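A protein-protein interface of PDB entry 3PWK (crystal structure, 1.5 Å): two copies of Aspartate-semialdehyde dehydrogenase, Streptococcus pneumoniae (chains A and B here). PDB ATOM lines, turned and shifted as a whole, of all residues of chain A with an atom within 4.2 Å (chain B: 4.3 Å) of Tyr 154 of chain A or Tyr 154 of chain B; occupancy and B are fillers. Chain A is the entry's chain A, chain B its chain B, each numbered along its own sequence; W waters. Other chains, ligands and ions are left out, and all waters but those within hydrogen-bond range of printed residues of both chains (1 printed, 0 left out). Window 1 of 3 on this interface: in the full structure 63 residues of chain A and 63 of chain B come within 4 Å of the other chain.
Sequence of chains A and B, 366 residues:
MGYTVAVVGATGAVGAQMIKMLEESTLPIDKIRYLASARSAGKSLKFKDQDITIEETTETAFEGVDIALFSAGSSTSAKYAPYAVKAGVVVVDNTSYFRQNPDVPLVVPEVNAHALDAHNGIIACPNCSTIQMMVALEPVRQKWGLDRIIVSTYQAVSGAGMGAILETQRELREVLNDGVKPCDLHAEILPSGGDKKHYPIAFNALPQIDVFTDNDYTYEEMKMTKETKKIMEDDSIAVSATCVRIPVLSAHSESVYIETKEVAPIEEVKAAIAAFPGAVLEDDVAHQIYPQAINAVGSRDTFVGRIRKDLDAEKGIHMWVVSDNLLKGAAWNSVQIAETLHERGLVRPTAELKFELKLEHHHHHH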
ATOM      1  N   SER A 152      15.366 -27.485  -9.639  1.00  0.00           N
ATOM      2  CA  SER A 152      15.091 -27.412  -8.207  1.00  0.00           C
ATOM      3  C   SER A 152      13.700 -27.954  -7.979  1.00  0.00           C
ATOM      4  O   SER A 152      12.747 -27.534  -8.660  1.00  0.00           O
ATOM      5  CB  SER A 152      15.151 -25.969  -7.725  1.00  0.00           C
ATOM      6  OG  SER A 152      16.472 -25.450  -7.842  1.00  0.00           O
ATOM      7  N   THR A 153      13.575 -28.933  -7.082  1.00  0.00           N
ATOM      8  CA  THR A 153      12.293 -29.604  -6.926  1.00  0.00           C
ATOM      9  C   THR A 153      11.532 -29.147  -5.672  1.00  0.00           C
ATOM     10  O   THR A 153      12.104 -28.570  -4.714  1.00  0.00           O
ATOM     11  CB  THR A 153      12.434 -31.143  -6.865  1.00  0.00           C
ATOM     12  OG1 THR A 153      12.960 -31.505  -5.590  1.00  0.00           O
ATOM     13  CG2 THR A 153      13.324 -31.704  -7.973  1.00  0.00           C
ATOM     14  N   TYR A 154      10.235 -29.445  -5.683  1.00  0.00           N
ATOM     15  CA  TYR A 154       9.296 -29.057  -4.632  1.00  0.00           C
ATOM     16  C   TYR A 154       8.479 -30.337  -4.418  1.00  0.00           C
ATOM     17  O   TYR A 154       7.396 -30.523  -5.002  1.00  0.00           O
ATOM     18  CB  TYR A 154       8.384 -27.898  -5.103  1.00  0.00           C
ATOM     19  CG  TYR A 154       9.090 -26.593  -5.467  1.00  0.00           C
ATOM     20  CD1 TYR A 154       8.822 -25.421  -4.747  1.00  0.00           C
ATOM     21  CD2 TYR A 154       9.956 -26.510  -6.574  1.00  0.00           C
ATOM     22  CE1 TYR A 154       9.440 -24.207  -5.077  1.00  0.00           C
ATOM     23  CE2 TYR A 154      10.604 -25.311  -6.901  1.00  0.00           C
ATOM     24  CZ  TYR A 154      10.364 -24.168  -6.152  1.00  0.00           C
ATOM     25  OH  TYR A 154      10.992 -23.001  -6.499  1.00  0.00           O
ATOM     26  N   GLN A 155       9.024 -31.248  -3.619  1.00  0.00           N
ATOM     27  CA  GLN A 155       8.529 -32.630  -3.597  1.00  0.00           C
ATOM     28  C   GLN A 155       7.565 -32.886  -2.459  1.00  0.00           C
ATOM     29  O   GLN A 155       7.763 -32.433  -1.318  1.00  0.00           O
ATOM     30  CB  GLN A 155       9.699 -33.625  -3.588  1.00  0.00           C
ATOM     31  CG  GLN A 155      10.358 -33.688  -4.974  1.00  0.00           C
ATOM     32  CD  GLN A 155      11.595 -34.567  -5.046  1.00  0.00           C
ATOM     33  OE1 GLN A 155      12.699 -34.072  -5.293  1.00  0.00           O
ATOM     34  NE2 GLN A 155      11.419 -35.881  -4.865  1.00  0.00           N
ATOM     35  N   ALA A 156       6.518 -33.637  -2.787  1.00  0.00           N
ATOM     36  CA  ALA A 156       5.473 -34.031  -1.846  1.00  0.00           C
ATOM     37  C   ALA A 156       5.943 -35.147  -0.906  1.00  0.00           C
ATOM     38  O   ALA A 156       6.784 -35.974  -1.272  1.00  0.00           O
ATOM     39  CB  ALA A 156       4.240 -34.493  -2.635  1.00  0.00           C
ATOM     40  N   VAL A 244      14.108 -30.792  -2.824  1.00  0.00           N
ATOM     41  CA  VAL A 244      13.593 -30.194  -1.585  1.00  0.00           C
ATOM     42  C   VAL A 244      12.206 -30.743  -1.269  1.00  0.00           C
ATOM     43  O   VAL A 244      11.348 -30.798  -2.158  1.00  0.00           O
ATOM     44  CB  VAL A 244      13.491 -28.643  -1.723  1.00  0.00           C
ATOM     45  CG1 VAL A 244      13.035 -27.992  -0.409  1.00  0.00           C
ATOM     46  CG2 VAL A 244      14.819 -28.052  -2.199  1.00  0.00           C
ATOM     47  N   ILE A 246       8.647 -30.245   0.566  1.00  0.00           N
ATOM     48  CA  ILE A 246       7.792 -29.157   1.036  1.00  0.00           C
ATOM     49  C   ILE A 246       6.496 -29.738   1.616  1.00  0.00           C
ATOM     50  O   ILE A 246       6.222 -30.916   1.421  1.00  0.00           O
ATOM     51  CB  ILE A 246       7.506 -28.096  -0.075  1.00  0.00           C
ATOM     52  CG1 ILE A 246       6.733 -28.705  -1.247  1.00  0.00           C
ATOM     53  CG2 ILE A 246       8.808 -27.419  -0.550  1.00  0.00           C
ATOM     54  CD1 ILE A 246       6.069 -27.614  -2.125  1.00  0.00           C
ATOM     55  N   HIS A 252       4.544 -33.732  -7.136  1.00  0.00           N
ATOM     56  CA  HIS A 252       5.817 -33.019  -7.135  1.00  0.00           C
ATOM     57  C   HIS A 252       5.769 -31.894  -8.146  1.00  0.00           C
ATOM     58  O   HIS A 252       5.199 -32.053  -9.238  1.00  0.00           O
ATOM     59  CB  HIS A 252       6.960 -33.933  -7.577  1.00  0.00           C
ATOM     60  CG  HIS A 252       7.294 -35.038  -6.616  1.00  0.00           C
ATOM     61  ND1 HIS A 252       6.882 -35.054  -5.301  1.00  0.00           N
ATOM     62  CD2 HIS A 252       8.065 -36.139  -6.781  1.00  0.00           C
ATOM     63  CE1 HIS A 252       7.367 -36.128  -4.700  1.00  0.00           C
ATOM     64  NE2 HIS A 252       8.093 -36.803  -5.577  1.00  0.00           N
ATOM     65  N   SER A 253       6.430 -30.784  -7.817  1.00  0.00           N
ATOM     66  CA  SER A 253       6.581 -29.671  -8.752  1.00  0.00           C
ATOM     67  C   SER A 253       8.060 -29.453  -8.981  1.00  0.00           C
ATOM     68  O   SER A 253       8.868 -29.697  -8.074  1.00  0.00           O
ATOM     69  CB  SER A 253       5.977 -28.382  -8.175  1.00  0.00           C
ATOM     70  OG  SER A 253       4.616 -28.602  -7.776  1.00  0.00           O
ATOM     71  N   SER A 255      10.975 -26.630 -10.782  1.00  0.00           N
ATOM     72  CA  SER A 255      11.431 -25.491 -11.557  1.00  0.00           C
ATOM     73  C   SER A 255      12.615 -26.006 -12.380  1.00  0.00           C
ATOM     74  O   SER A 255      13.656 -26.379 -11.815  1.00  0.00           O
ATOM     75  CB  SER A 255      11.838 -24.365 -10.606  1.00  0.00           C
ATOM     76  OG  SER A 255      12.407 -23.299 -11.347  1.00  0.00           O
ATOM     77  N   TRP A 320       7.940 -24.952 -15.534  1.00  0.00           N
ATOM     78  CA  TRP A 320       7.390 -25.476 -14.287  1.00  0.00           C
ATOM     79  C   TRP A 320       6.652 -26.762 -14.630  1.00  0.00           C
ATOM     80  O   TRP A 320       5.775 -26.764 -15.526  1.00  0.00           O
ATOM     81  CB  TRP A 320       6.416 -24.437 -13.730  1.00  0.00           C
ATOM     82  CG  TRP A 320       5.770 -24.770 -12.411  1.00  0.00           C
ATOM     83  CD1 TRP A 320       4.449 -25.029 -12.187  1.00  0.00           C
ATOM     84  CD2 TRP A 320       6.410 -24.793 -11.127  1.00  0.00           C
ATOM     85  NE1 TRP A 320       4.221 -25.213 -10.839  1.00  0.00           N
ATOM     86  CE2 TRP A 320       5.410 -25.067 -10.165  1.00  0.00           C
ATOM     87  CE3 TRP A 320       7.729 -24.593 -10.696  1.00  0.00           C
ATOM     88  CZ2 TRP A 320       5.698 -25.170  -8.793  1.00  0.00           C
ATOM     89  CZ3 TRP A 320       8.016 -24.703  -9.331  1.00  0.00           C
ATOM     90  CH2 TRP A 320       7.006 -24.967  -8.404  1.00  0.00           C
ATOM     91  N   SER B 152      15.508 -20.262  -7.874  1.00  0.00           N
ATOM     92  CA  SER B 152      14.126 -20.705  -7.682  1.00  0.00           C
ATOM     93  C   SER B 152      13.781 -20.535  -6.219  1.00  0.00           C
ATOM     94  O   SER B 152      14.521 -21.006  -5.357  1.00  0.00           O
ATOM     95  CB  SER B 152      13.945 -22.172  -8.097  1.00  0.00           C
ATOM     96  OG  SER B 152      14.168 -22.314  -9.502  1.00  0.00           O
ATOM     97  N   THR B 153      12.698 -19.811  -5.944  1.00  0.00           N
ATOM     98  CA  THR B 153      12.371 -19.484  -4.562  1.00  0.00           C
ATOM     99  C   THR B 153      11.263 -20.354  -3.992  1.00  0.00           C
ATOM    100  O   THR B 153      10.448 -20.956  -4.739  1.00  0.00           O
ATOM    101  CB  THR B 153      11.983 -17.995  -4.389  1.00  0.00           C
ATOM    102  OG1 THR B 153      10.662 -17.810  -4.905  1.00  0.00           O
ATOM    103  CG2 THR B 153      12.976 -17.045  -5.109  1.00  0.00           C
ATOM    104  N   TYR B 154      11.208 -20.360  -2.663  1.00  0.00           N
ATOM    105  CA  TYR B 154      10.246 -21.140  -1.894  1.00  0.00           C
ATOM    106  C   TYR B 154       9.753 -20.143  -0.841  1.00  0.00           C
ATOM    107  O   TYR B 154      10.275 -20.086   0.297  1.00  0.00           O
ATOM    108  CB  TYR B 154      10.953 -22.325  -1.214  1.00  0.00           C
ATOM    109  CG  TYR B 154      11.590 -23.346  -2.154  1.00  0.00           C
ATOM    110  CD1 TYR B 154      11.129 -24.670  -2.182  1.00  0.00           C
ATOM    111  CD2 TYR B 154      12.692 -23.006  -2.970  1.00  0.00           C
ATOM    112  CE1 TYR B 154      11.702 -25.620  -3.023  1.00  0.00           C
ATOM    113  CE2 TYR B 154      13.283 -23.944  -3.826  1.00  0.00           C
ATOM    114  CZ  TYR B 154      12.788 -25.249  -3.843  1.00  0.00           C
ATOM    115  OH  TYR B 154      13.384 -26.153  -4.688  1.00  0.00           O
ATOM    116  N   GLN B 155       8.783 -19.316  -1.232  1.00  0.00           N
ATOM    117  CA  GLN B 155       8.435 -18.142  -0.448  1.00  0.00           C
ATOM    118  C   GLN B 155       7.253 -18.349   0.485  1.00  0.00           C
ATOM    119  O   GLN B 155       6.248 -18.963   0.126  1.00  0.00           O
ATOM    120  CB  GLN B 155       8.221 -16.920  -1.367  1.00  0.00           C
ATOM    121  CG  GLN B 155       9.574 -16.450  -1.957  1.00  0.00           C
ATOM    122  CD  GLN B 155       9.454 -15.294  -2.942  1.00  0.00           C
ATOM    123  OE1 GLN B 155       9.817 -15.430  -4.107  1.00  0.00           O
ATOM    124  NE2 GLN B 155       8.945 -14.156  -2.477  1.00  0.00           N
ATOM    125  N   ALA B 156       7.398 -17.781   1.680  1.00  0.00           N
ATOM    126  CA  ALA B 156       6.387 -17.805   2.745  1.00  0.00           C
ATOM    127  C   ALA B 156       5.248 -16.825   2.474  1.00  0.00           C
ATOM    128  O   ALA B 156       5.443 -15.781   1.845  1.00  0.00           O
ATOM    129  CB  ALA B 156       7.050 -17.455   4.060  1.00  0.00           C
ATOM    130  N   VAL B 244       8.112 -18.842  -6.293  1.00  0.00           N
ATOM    131  CA  VAL B 244       7.026 -19.792  -6.003  1.00  0.00           C
ATOM    132  C   VAL B 244       6.593 -19.622  -4.564  1.00  0.00           C
ATOM    133  O   VAL B 244       7.444 -19.573  -3.672  1.00  0.00           O
ATOM    134  CB  VAL B 244       7.499 -21.249  -6.222  1.00  0.00           C
ATOM    135  CG1 VAL B 244       6.349 -22.231  -6.025  1.00  0.00           C
ATOM    136  CG2 VAL B 244       8.144 -21.413  -7.621  1.00  0.00           C
ATOM    137  N   ILE B 246       4.943 -21.241  -1.283  1.00  0.00           N
ATOM    138  CA  ILE B 246       4.683 -22.565  -0.701  1.00  0.00           C
ATOM    139  C   ILE B 246       3.976 -22.434   0.652  1.00  0.00           C
ATOM    140  O   ILE B 246       3.878 -21.307   1.179  1.00  0.00           O
ATOM    141  CB  ILE B 246       5.987 -23.417  -0.583  1.00  0.00           C
ATOM    142  CG1 ILE B 246       7.042 -22.746   0.332  1.00  0.00           C
ATOM    143  CG2 ILE B 246       6.586 -23.688  -1.970  1.00  0.00           C
ATOM    144  CD1 ILE B 246       8.090 -23.765   0.862  1.00  0.00           C
ATOM    145  N   HIS B 252      11.619 -17.219   3.888  1.00  0.00           N
ATOM    146  CA  HIS B 252      11.808 -17.628   2.498  1.00  0.00           C
ATOM    147  C   HIS B 252      13.053 -18.501   2.367  1.00  0.00           C
ATOM    148  O   HIS B 252      14.059 -18.265   3.040  1.00  0.00           O
ATOM    149  CB  HIS B 252      12.049 -16.422   1.581  1.00  0.00           C
ATOM    150  CG  HIS B 252      10.881 -15.489   1.449  1.00  0.00           C
ATOM    151  ND1 HIS B 252       9.583 -15.826   1.787  1.00  0.00           N
ATOM    152  CD2 HIS B 252      10.827 -14.221   0.970  1.00  0.00           C
ATOM    153  CE1 HIS B 252       8.786 -14.802   1.531  1.00  0.00           C
ATOM    154  NE2 HIS B 252       9.517 -13.815   1.035  1.00  0.00           N
ATOM    155  N   SER B 253      12.973 -19.506   1.507  1.00  0.00           N
ATOM    156  CA  SER B 253      14.130 -20.323   1.157  1.00  0.00           C
ATOM    157  C   SER B 253      14.394 -20.152  -0.329  1.00  0.00           C
ATOM    158  O   SER B 253      13.455 -19.943  -1.115  1.00  0.00           O
ATOM    159  CB  SER B 253      13.854 -21.801   1.451  1.00  0.00           C
ATOM    160  OG  SER B 253      13.352 -21.991   2.779  1.00  0.00           O
ATOM    161  N   SER B 255      16.778 -21.779  -3.714  1.00  0.00           N
ATOM    162  CA  SER B 255      17.775 -22.624  -4.384  1.00  0.00           C
ATOM    163  C   SER B 255      18.487 -21.698  -5.354  1.00  0.00           C
ATOM    164  O   SER B 255      17.888 -21.234  -6.322  1.00  0.00           O
ATOM    165  CB  SER B 255      17.094 -23.795  -5.104  1.00  0.00           C
ATOM    166  OG  SER B 255      18.070 -24.570  -5.776  1.00  0.00           O
ATOM    167  N   TRP B 320      21.761 -23.088  -0.812  1.00  0.00           N
ATOM    168  CA  TRP B 320      20.416 -22.970  -0.239  1.00  0.00           C
ATOM    169  C   TRP B 320      20.480 -21.822   0.768  1.00  0.00           C
ATOM    170  O   TRP B 320      21.311 -21.848   1.667  1.00  0.00           O
ATOM    171  CB  TRP B 320      20.095 -24.286   0.476  1.00  0.00           C
ATOM    172  CG  TRP B 320      18.718 -24.399   1.085  1.00  0.00           C
ATOM    173  CD1 TRP B 320      18.421 -24.502   2.416  1.00  0.00           C
ATOM    174  CD2 TRP B 320      17.473 -24.510   0.381  1.00  0.00           C
ATOM    175  NE1 TRP B 320      17.063 -24.656   2.588  1.00  0.00           N
ATOM    176  CE2 TRP B 320      16.454 -24.662   1.360  1.00  0.00           C
ATOM    177  CE3 TRP B 320      17.117 -24.486  -0.981  1.00  0.00           C
ATOM    178  CZ2 TRP B 320      15.095 -24.791   1.028  1.00  0.00           C
ATOM    179  CZ3 TRP B 320      15.760 -24.611  -1.319  1.00  0.00           C
ATOM    180  CH2 TRP B 320      14.763 -24.760  -0.315  1.00  0.00           C
HETATM  181  O   HOH W   1      16.516 -23.643  -9.846  1.00  0.00           O
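Water W1 bridges OG of Ser 152 of chain A and OG of Ser 152 of chain B.
The side-chain hydroxyl of Ser 255 of chain B is in hydrogen-bond range of the side-chain hydroxyl of Ser 152 of chain A (2.8 Å).
The side-chain hydroxyl (OG) of Ser 255 of chain A sits at hydrogen-bond distance from the side-chain hydroxyl (OG) of Ser 152 of chain B (2.7 Å).
The side-chain hydroxyl (OH) of Tyr 154 of chain B lies within hydrogen-bond range of the backbone carbonyl oxygen (O) of Thr 153 of chain A (2.7 Å).
O of Thr 153 of chain B sits at hydrogen-bond distance from OH of Tyr 154 of chain A, 2.8 Å away.
Hydrophobic or aromatic side chains of chain A that line the printed part of chain B: Tyr 154, Val 244, Ile 246 and Trp 320.
Among the printed residues, no Asp or Glu carboxylate lies within 4 Å of a Lys or Arg side-chain nitrogen of the other chain.
Of the printed residues of chain B, Tyr 154 of chain A touches Ser 152, Thr 153, Tyr 154, Val 244 and Ile 246.
Tyr 154 of chain B touches five residues of chain A.
Printed residues of chain B within 4 Å of Ser 152 of chain A: Tyr 154 (3.5 Å) and Ser 255 (2.8 Å).
Of the printed residues of chain A, Trp 320 of chain B touches Val 244 (3.7 Å).
Of the printed residues of chain A, Val 244 of chain B touches Tyr 154 and Trp 320.
Of the printed residues of chain A, Ile 246 of chain B touches Tyr 154 (3.96 Å) and Ile 246 (3.96 Å).
Ala 156 of chain A touches none of the printed residues of chain B.
Tyr 154 of chain B touches Ser 152 of chain A (OH to CB, 3.5 Å).
Ser 152 of chain B touches Tyr 154 of chain A.
Tyr 154 of chain A touches Tyr 154 of chain B.
Val 244 of chain B touches Tyr 154 of chain A.
Ile 246 of chain B touches Tyr 154 of chain A (CG2 to CD1, 3.96 Å).
Val 244 of chain A touches Tyr 154 of chain B.
Trp 320 of chain B touches Val 244 of chain A.
Ile 246 of chain A touches Tyr 154 of chain B (CG2 to CD1, 3.95 Å).
Ile 246 of chain A touches Ile 246 of chain B (CD1 to CG2, 3.96 Å).
Val 244 of chain B touches Trp 320 of chain A (CG1 to CH2, 3.7 Å).
The side-chain hydroxyl (OG1) of Thr 153 of chain B lies within hydrogen-bond range of the backbone NH (N) of Val 244 of chain B (3.1 Å).
O of Gln 155 of chain A sits at hydrogen-bond distance from N of Ile 246 of chain A (3.0 Å).
OG1 of Thr 153 of chain B sits at hydrogen-bond distance from OE1 of Gln 155 of chain B (2.6 Å).
The backbone carbonyl oxygen (O) of Ser 152 of chain B lies within hydrogen-bond range of the backbone NH (N) of Ser 255 of chain B, at 2.9 Å.
N of Tyr 154 of chain B lies within hydrogen-bond range of O of Ser 253 of chain B, 2.8 Å away.
The backbone NH of Gln 155 of chain B lies within hydrogen-bond range of the backbone carbonyl oxygen of Val 244 of chain B, at 2.8 Å.
Thr 153 of chain A touches Tyr 154 of chain B, and with the chains exchanged Tyr 154 of chain A touches Thr 153 of chain B.
Tyr 154 of chain A touches Val 244 of chain B, and with the chains exchanged Val 244 of chain A touches Tyr 154 of chain B.
Val 244 of chain A touches Trp 320 of chain B, and with the chains exchanged Trp 320 of chain A touches Val 244 of chain B.
Ile 246 of chain B touches its own counterpart, Ile 246 of chain A.
Positions printed for both chains: 152, 153, 154, 155, 156, 244, 246, 252, 253, 255 and 320.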
